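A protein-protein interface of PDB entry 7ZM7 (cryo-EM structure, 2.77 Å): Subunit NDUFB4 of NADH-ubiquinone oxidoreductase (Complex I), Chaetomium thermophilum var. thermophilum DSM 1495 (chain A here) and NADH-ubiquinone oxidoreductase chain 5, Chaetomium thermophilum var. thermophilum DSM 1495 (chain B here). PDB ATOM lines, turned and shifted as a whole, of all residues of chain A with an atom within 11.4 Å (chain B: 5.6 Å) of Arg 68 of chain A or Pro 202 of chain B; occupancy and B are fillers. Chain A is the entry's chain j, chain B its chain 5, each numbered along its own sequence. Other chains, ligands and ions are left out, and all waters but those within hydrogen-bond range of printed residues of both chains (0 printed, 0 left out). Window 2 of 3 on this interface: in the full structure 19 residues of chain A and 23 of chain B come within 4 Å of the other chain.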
ATOM      1  N   ASP A  62      37.904   1.714  15.901  1.00  0.00           N
ATOM      2  CA  ASP A  62      36.970   1.618  14.744  1.00  0.00           C
ATOM      3  C   ASP A  62      35.881   0.604  15.120  1.00  0.00           C
ATOM      4  O   ASP A  62      36.243  -0.472  15.619  1.00  0.00           O
ATOM      5  CB  ASP A  62      37.697   1.225  13.459  1.00  0.00           C
ATOM      6  CG  ASP A  62      36.798   1.151  12.238  1.00  0.00           C
ATOM      7  OD1 ASP A  62      35.989   2.076  12.051  1.00  0.00           O
ATOM      8  OD2 ASP A  62      36.916   0.165  11.486  1.00  0.00           O
ATOM      9  N   LEU A  63      34.605   0.943  14.919  1.00  0.00           N
ATOM     10  CA  LEU A  63      33.483   0.016  15.232  1.00  0.00           C
ATOM     11  C   LEU A  63      32.971  -0.633  13.947  1.00  0.00           C
ATOM     12  O   LEU A  63      32.055  -1.452  14.050  1.00  0.00           O
ATOM     13  CB  LEU A  63      32.339   0.822  15.854  1.00  0.00           C
ATOM     14  CG  LEU A  63      32.608   1.517  17.185  1.00  0.00           C
ATOM     15  CD1 LEU A  63      31.319   2.121  17.718  1.00  0.00           C
ATOM     16  CD2 LEU A  63      33.176   0.541  18.197  1.00  0.00           C
ATOM     17  N   ARG A  64      33.611  -0.386  12.807  1.00  0.00           N
ATOM     18  CA  ARG A  64      33.053  -0.844  11.503  1.00  0.00           C
ATOM     19  C   ARG A  64      33.207  -2.352  11.293  1.00  0.00           C
ATOM     20  O   ARG A  64      34.360  -2.800  11.132  1.00  0.00           O
ATOM     21  CB  ARG A  64      33.563   0.012  10.338  1.00  0.00           C
ATOM     22  CG  ARG A  64      32.997  -0.367   8.975  1.00  0.00           C
ATOM     23  CD  ARG A  64      31.488  -0.542   8.909  1.00  0.00           C
ATOM     24  NE  ARG A  64      30.712   0.664   9.161  1.00  0.00           N
ATOM     25  CZ  ARG A  64      30.155   1.422   8.223  1.00  0.00           C
ATOM     26  NH1 ARG A  64      29.468   2.497   8.565  1.00  0.00           N
ATOM     27  NH2 ARG A  64      30.281   1.100   6.948  1.00  0.00           N
ATOM     28  N   ALA A  65      32.099  -3.098  11.299  1.00  0.00           N
ATOM     29  CA  ALA A  65      32.145  -4.515  10.969  1.00  0.00           C
ATOM     30  C   ALA A  65      32.790  -5.379  12.049  1.00  0.00           C
ATOM     31  O   ALA A  65      32.832  -6.604  11.910  1.00  0.00           O
ATOM     32  CB  ALA A  65      32.853  -4.715   9.630  1.00  0.00           C
ATOM     33  N   LYS A  66      33.264  -4.767  13.133  1.00  0.00           N
ATOM     34  CA  LYS A  66      33.926  -5.511  14.197  1.00  0.00           C
ATOM     35  C   LYS A  66      32.954  -6.463  14.875  1.00  0.00           C
ATOM     36  O   LYS A  66      31.830  -6.088  15.200  1.00  0.00           O
ATOM     37  CB  LYS A  66      34.514  -4.552  15.228  1.00  0.00           C
ATOM     38  CG  LYS A  66      35.465  -3.536  14.661  1.00  0.00           C
ATOM     39  CD  LYS A  66      36.860  -4.112  14.564  1.00  0.00           C
ATOM     40  CE  LYS A  66      37.897  -3.034  14.385  1.00  0.00           C
ATOM     41  NZ  LYS A  66      37.628  -2.221  13.191  1.00  0.00           N
ATOM     42  N   ARG A  67      33.392  -7.707  15.054  1.00  0.00           N
ATOM     43  CA  ARG A  67      32.523  -8.732  15.674  1.00  0.00           C
ATOM     44  C   ARG A  67      33.162  -9.206  16.975  1.00  0.00           C
ATOM     45  O   ARG A  67      34.167  -8.607  17.393  1.00  0.00           O
ATOM     46  CB  ARG A  67      32.378  -9.934  14.743  1.00  0.00           C
ATOM     47  CG  ARG A  67      31.492  -9.677  13.535  1.00  0.00           C
ATOM     48  CD  ARG A  67      31.219 -10.966  12.789  1.00  0.00           C
ATOM     49  NE  ARG A  67      32.438 -11.589  12.298  1.00  0.00           N
ATOM     50  CZ  ARG A  67      32.916 -11.435  11.071  1.00  0.00           C
ATOM     51  NH1 ARG A  67      32.270 -10.679  10.199  1.00  0.00           N
ATOM     52  NH2 ARG A  67      34.033 -12.044  10.715  1.00  0.00           N
ATOM     53  N   ARG A  68      32.580 -10.232  17.595  1.00  0.00           N
ATOM     54  CA  ARG A  68      33.171 -10.811  18.827  1.00  0.00           C
ATOM     55  C   ARG A  68      34.448 -11.572  18.462  1.00  0.00           C
ATOM     56  O   ARG A  68      34.447 -12.258  17.426  1.00  0.00           O
ATOM     57  CB  ARG A  68      32.135 -11.674  19.546  1.00  0.00           C
ATOM     58  CG  ARG A  68      31.622 -11.034  20.829  1.00  0.00           C
ATOM     59  CD  ARG A  68      30.611 -11.864  21.593  1.00  0.00           C
ATOM     60  NE  ARG A  68      29.677 -12.499  20.680  1.00  0.00           N
ATOM     61  CZ  ARG A  68      29.713 -13.780  20.341  1.00  0.00           C
ATOM     62  NH1 ARG A  68      28.826 -14.253  19.486  1.00  0.00           N
ATOM     63  NH2 ARG A  68      30.628 -14.582  20.852  1.00  0.00           N
ATOM     64  N   GLY A  69      35.486 -11.461  19.290  1.00  0.00           N
ATOM     65  CA  GLY A  69      36.772 -12.111  18.983  1.00  0.00           C
ATOM     66  C   GLY A  69      37.708 -11.131  18.313  1.00  0.00           C
ATOM     67  O   GLY A  69      38.919 -11.409  18.265  1.00  0.00           O
ATOM     68  N   ASP A  70      37.160 -10.023  17.805  1.00  0.00           N
ATOM     69  CA  ASP A  70      37.988  -8.971  17.159  1.00  0.00           C
ATOM     70  C   ASP A  70      38.089  -7.835  18.178  1.00  0.00           C
ATOM     71  O   ASP A  70      37.381  -7.915  19.197  1.00  0.00           O
ATOM     72  CB  ASP A  70      37.359  -8.502  15.847  1.00  0.00           C
ATOM     73  CG  ASP A  70      38.356  -7.905  14.870  1.00  0.00           C
ATOM     74  OD1 ASP A  70      39.567  -7.988  15.147  1.00  0.00           O
ATOM     75  OD2 ASP A  70      37.912  -7.363  13.839  1.00  0.00           O
ATOM     76  N   LEU A  71      38.942  -6.838  17.941  1.00  0.00           N
ATOM     77  CA  LEU A  71      39.112  -5.771  18.963  1.00  0.00           C
ATOM     78  C   LEU A  71      38.730  -4.417  18.359  1.00  0.00           C
ATOM     79  O   LEU A  71      39.072  -4.182  17.190  1.00  0.00           O
ATOM     80  CB  LEU A  71      40.562  -5.767  19.455  1.00  0.00           C
ATOM     81  CG  LEU A  71      40.861  -6.710  20.618  1.00  0.00           C
ATOM     82  CD1 LEU A  71      42.285  -6.520  21.116  1.00  0.00           C
ATOM     83  CD2 LEU A  71      39.872  -6.492  21.753  1.00  0.00           C
ATOM     84  N   ILE A  72      38.041  -3.572  19.129  1.00  0.00           N
ATOM     85  CA  ILE A  72      37.658  -2.211  18.647  1.00  0.00           C
ATOM     86  C   ILE A  72      38.940  -1.428  18.374  1.00  0.00           C
ATOM     87  O   ILE A  72      38.997  -0.722  17.350  1.00  0.00           O
ATOM     88  CB  ILE A  72      36.789  -1.482  19.692  1.00  0.00           C
ATOM     89  CG1 ILE A  72      35.514  -2.256  20.030  1.00  0.00           C
ATOM     90  CG2 ILE A  72      36.485  -0.059  19.256  1.00  0.00           C
ATOM     91  CD1 ILE A  72      34.663  -1.581  21.075  1.00  0.00           C
ATOM     92  N   PHE B 198      18.941  -6.645  14.897  1.00  0.00           N
ATOM     93  CA  PHE B 198      18.695  -7.804  15.734  1.00  0.00           C
ATOM     94  C   PHE B 198      19.172  -9.089  15.077  1.00  0.00           C
ATOM     95  O   PHE B 198      19.629  -9.997  15.772  1.00  0.00           O
ATOM     96  CB  PHE B 198      17.214  -7.872  16.078  1.00  0.00           C
ATOM     97  CG  PHE B 198      16.680  -6.607  16.663  1.00  0.00           C
ATOM     98  CD1 PHE B 198      17.491  -5.774  17.408  1.00  0.00           C
ATOM     99  CD2 PHE B 198      15.367  -6.243  16.471  1.00  0.00           C
ATOM    100  CE1 PHE B 198      17.004  -4.609  17.927  1.00  0.00           C
ATOM    101  CE2 PHE B 198      14.882  -5.073  17.004  1.00  0.00           C
ATOM    102  CZ  PHE B 198      15.702  -4.264  17.730  1.00  0.00           C
ATOM    103  N   SER B 199      19.116  -9.177  13.752  1.00  0.00           N
ATOM    104  CA  SER B 199      19.683 -10.344  13.094  1.00  0.00           C
ATOM    105  C   SER B 199      21.182 -10.450  13.337  1.00  0.00           C
ATOM    106  O   SER B 199      21.725 -11.554  13.367  1.00  0.00           O
ATOM    107  CB  SER B 199      19.388 -10.305  11.602  1.00  0.00           C
ATOM    108  OG  SER B 199      19.828  -9.096  11.036  1.00  0.00           O
ATOM    109  N   LEU B 200      21.853  -9.328  13.544  1.00  0.00           N
ATOM    110  CA  LEU B 200      23.300  -9.298  13.637  1.00  0.00           C
ATOM    111  C   LEU B 200      23.834  -9.205  15.050  1.00  0.00           C
ATOM    112  O   LEU B 200      25.025  -9.445  15.244  1.00  0.00           O
ATOM    113  CB  LEU B 200      23.847  -8.119  12.844  1.00  0.00           C
ATOM    114  CG  LEU B 200      23.829  -8.287  11.342  1.00  0.00           C
ATOM    115  CD1 LEU B 200      24.448  -7.071  10.757  1.00  0.00           C
ATOM    116  CD2 LEU B 200      24.603  -9.513  10.964  1.00  0.00           C
ATOM    117  N   ALA B 201      22.998  -8.865  16.027  1.00  0.00           N
ATOM    118  CA  ALA B 201      23.495  -8.557  17.367  1.00  0.00           C
ATOM    119  C   ALA B 201      24.282  -9.675  18.050  1.00  0.00           C
ATOM    120  O   ALA B 201      25.297  -9.358  18.695  1.00  0.00           O
ATOM    121  CB  ALA B 201      22.329  -8.116  18.254  1.00  0.00           C
ATOM    122  N   PRO B 202      23.886 -10.978  18.028  1.00  0.00           N
ATOM    123  CA  PRO B 202      24.624 -11.997  18.791  1.00  0.00           C
ATOM    124  C   PRO B 202      26.127 -12.029  18.485  1.00  0.00           C
ATOM    125  O   PRO B 202      26.877 -12.424  19.350  1.00  0.00           O
ATOM    126  CB  PRO B 202      24.046 -13.336  18.321  1.00  0.00           C
ATOM    127  CG  PRO B 202      22.661 -13.011  17.835  1.00  0.00           C
ATOM    128  CD  PRO B 202      22.752 -11.599  17.306  1.00  0.00           C
ATOM    129  N   TYR B 203      26.525 -11.620  17.279  1.00  0.00           N
ATOM    130  CA  TYR B 203      27.945 -11.729  16.857  1.00  0.00           C
ATOM    131  C   TYR B 203      28.702 -10.415  17.050  1.00  0.00           C
ATOM    132  O   TYR B 203      29.920 -10.413  16.848  1.00  0.00           O
ATOM    133  CB  TYR B 203      27.951 -12.162  15.391  1.00  0.00           C
ATOM    134  CG  TYR B 203      26.791 -13.069  15.080  1.00  0.00           C
ATOM    135  CD1 TYR B 203      26.790 -14.382  15.511  1.00  0.00           C
ATOM    136  CD2 TYR B 203      25.673 -12.608  14.405  1.00  0.00           C
ATOM    137  CE1 TYR B 203      25.726 -15.228  15.262  1.00  0.00           C
ATOM    138  CE2 TYR B 203      24.595 -13.437  14.152  1.00  0.00           C
ATOM    139  CZ  TYR B 203      24.625 -14.753  14.578  1.00  0.00           C
ATOM    140  OH  TYR B 203      23.574 -15.584  14.338  1.00  0.00           O
ATOM    141  N   ILE B 204      28.019  -9.347  17.453  1.00  0.00           N
ATOM    142  CA  ILE B 204      28.680  -8.009  17.540  1.00  0.00           C
ATOM    143  C   ILE B 204      29.644  -7.969  18.732  1.00  0.00           C
ATOM    144  O   ILE B 204      29.398  -8.695  19.711  1.00  0.00           O
ATOM    145  CB  ILE B 204      27.618  -6.892  17.543  1.00  0.00           C
ATOM    146  CG1 ILE B 204      26.851  -6.888  16.220  1.00  0.00           C
ATOM    147  CG2 ILE B 204      28.212  -5.522  17.835  1.00  0.00           C
ATOM    148  CD1 ILE B 204      27.729  -7.154  15.020  1.00  0.00           C
ATOM    149  N   ASN B 205      30.681  -7.130  18.660  1.00  0.00           N
ATOM    150  CA  ASN B 205      31.694  -7.032  19.742  1.00  0.00           C
ATOM    151  C   ASN B 205      30.973  -6.691  21.049  1.00  0.00           C
ATOM    152  O   ASN B 205      30.195  -5.724  21.055  1.00  0.00           O
ATOM    153  CB  ASN B 205      32.730  -5.959  19.410  1.00  0.00           C
ATOM    154  CG  ASN B 205      33.986  -6.060  20.245  1.00  0.00           C
ATOM    155  OD1 ASN B 205      34.790  -6.967  20.054  1.00  0.00           O
ATOM    156  ND2 ASN B 205      34.162  -5.135  21.171  1.00  0.00           N
ATOM    157  N   SER B 206      31.212  -7.474  22.105  1.00  0.00           N
ATOM    158  CA  SER B 206      30.510  -7.255  23.392  1.00  0.00           C
ATOM    159  C   SER B 206      30.682  -5.803  23.842  1.00  0.00           C
ATOM    160  O   SER B 206      29.715  -5.255  24.400  1.00  0.00           O
ATOM    161  CB  SER B 206      30.986  -8.209  24.441  1.00  0.00           C
ATOM    162  OG  SER B 206      30.159  -8.126  25.590  1.00  0.00           O
ATOM    163  N   PRO B 265      16.155  -7.607  21.503  1.00  0.00           N
ATOM    164  CA  PRO B 265      16.980  -8.601  20.815  1.00  0.00           C
ATOM    165  C   PRO B 265      18.406  -8.148  20.607  1.00  0.00           C
ATOM    166  O   PRO B 265      19.156  -8.823  19.903  1.00  0.00           O
ATOM    167  CB  PRO B 265      16.261  -8.782  19.468  1.00  0.00           C
ATOM    168  CG  PRO B 265      14.978  -8.140  19.616  1.00  0.00           C
ATOM    169  CD  PRO B 265      15.177  -7.041  20.565  1.00  0.00           C
ATOM    170  N   TYR B 269      22.202  -8.960  24.922  1.00  0.00           N
ATOM    171  CA  TYR B 269      23.563  -9.402  24.690  1.00  0.00           C
ATOM    172  C   TYR B 269      24.576  -8.570  25.450  1.00  0.00           C
ATOM    173  O   TYR B 269      25.742  -8.506  25.057  1.00  0.00           O
ATOM    174  CB  TYR B 269      23.859  -9.408  23.193  1.00  0.00           C
ATOM    175  CG  TYR B 269      23.220 -10.587  22.515  1.00  0.00           C
ATOM    176  CD1 TYR B 269      23.756 -11.848  22.645  1.00  0.00           C
ATOM    177  CD2 TYR B 269      22.066 -10.442  21.759  1.00  0.00           C
ATOM    178  CE1 TYR B 269      23.169 -12.930  22.052  1.00  0.00           C
ATOM    179  CE2 TYR B 269      21.476 -11.521  21.154  1.00  0.00           C
ATOM    180  CZ  TYR B 269      22.028 -12.762  21.311  1.00  0.00           C
ATOM    181  OH  TYR B 269      21.443 -13.841  20.709  1.00  0.00           O
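Among the printed residues, merely in contact across the chains: Arg 67 of chain A with Tyr 203 of chain B (3.3 Å), Ile 72 of chain A with Asn 205 of chain B (3.4 Å), Arg 68 of chain A with Ile 204 of chain B (3.4 Å), Arg 68 of chain A with Asn 205 of chain B (3.8 Å), Lys 66 of chain A with Asn 205 of chain B (3.8 Å) and Arg 68 of chain A with Ser 206 of chain B (3.8 Å).
The backbone carbonyl oxygen of Arg 67 of chain A sits close to the side-chain amide oxygen of Asn 205 of chain B, at 3.2 Å. The guanidinium group of Arg 68 of chain A is in hydrogen-bond range of the backbone carbonyl oxygen of Pro 202 of chain B. The backbone carbonyl oxygen of Asp 70 of chain A lies close to the side-chain amide oxygen of Asn 205 of chain B (2.9 Å). The backbone NH (N) of Arg 68 of chain A sits at hydrogen-bond distance from the backbone carbonyl oxygen (O) of Tyr 203 of chain B, at 2.8 Å.
Arg 68 of chain A touches just these residues of chain B: Pro 202 (2.7 Å), Tyr 203 (2.8 Å), Ile 204 (3.4 Å), Asn 205 (3.8 Å) and Ser 206 (3.8 Å). Pro 202 of chain B touches one residue of chain A. Tyr 203 of chain B touches just these residues of chain A: Arg 67 (3.3 Å) and Arg 68 (2.8 Å). Ile 204 of chain B touches just one residue of chain A: Arg 68 (3.4 Å). Of the printed residues of chain A, Ser 206 of chain B touches Arg 68. Printed residues of chain B within 4 Å of Lys 66 of chain A: Asn 205. Printed residues of chain B within 4 Å of Asp 70 of chain A: Asn 205 (2.9 Å). Printed residues of chain B within 4 Å of Ile 72 of chain A: Asn 205. Printed residues of chain B within 4 Å of Arg 67 of chain A: Tyr 203 and Asn 205. Tyr 269 of chain B touches none of the printed residues of chain A.
The backbone NH (N) of Asp 62 of chain A sits at hydrogen-bond distance from the backbone carbonyl oxygen (O) of Ile 72 of chain A, 3.0 Å away. OD2 of Asp 62 of chain A lies within salt-bridge range of NZ of Lys 66 of chain A, 3.0 Å away.
Of the 11 printed residues of chain B, 5 touch a printed residue of chain A. Printed residues of chain B that touch a printed residue of chain A: Pro 202, Tyr 203, Ile 204, Asn 205 and Ser 206. Hydrophobic or aromatic side chains of chain A that line the printed part of chain B: Ile 72. Among the printed residues, 10 pairs touch across the chains.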
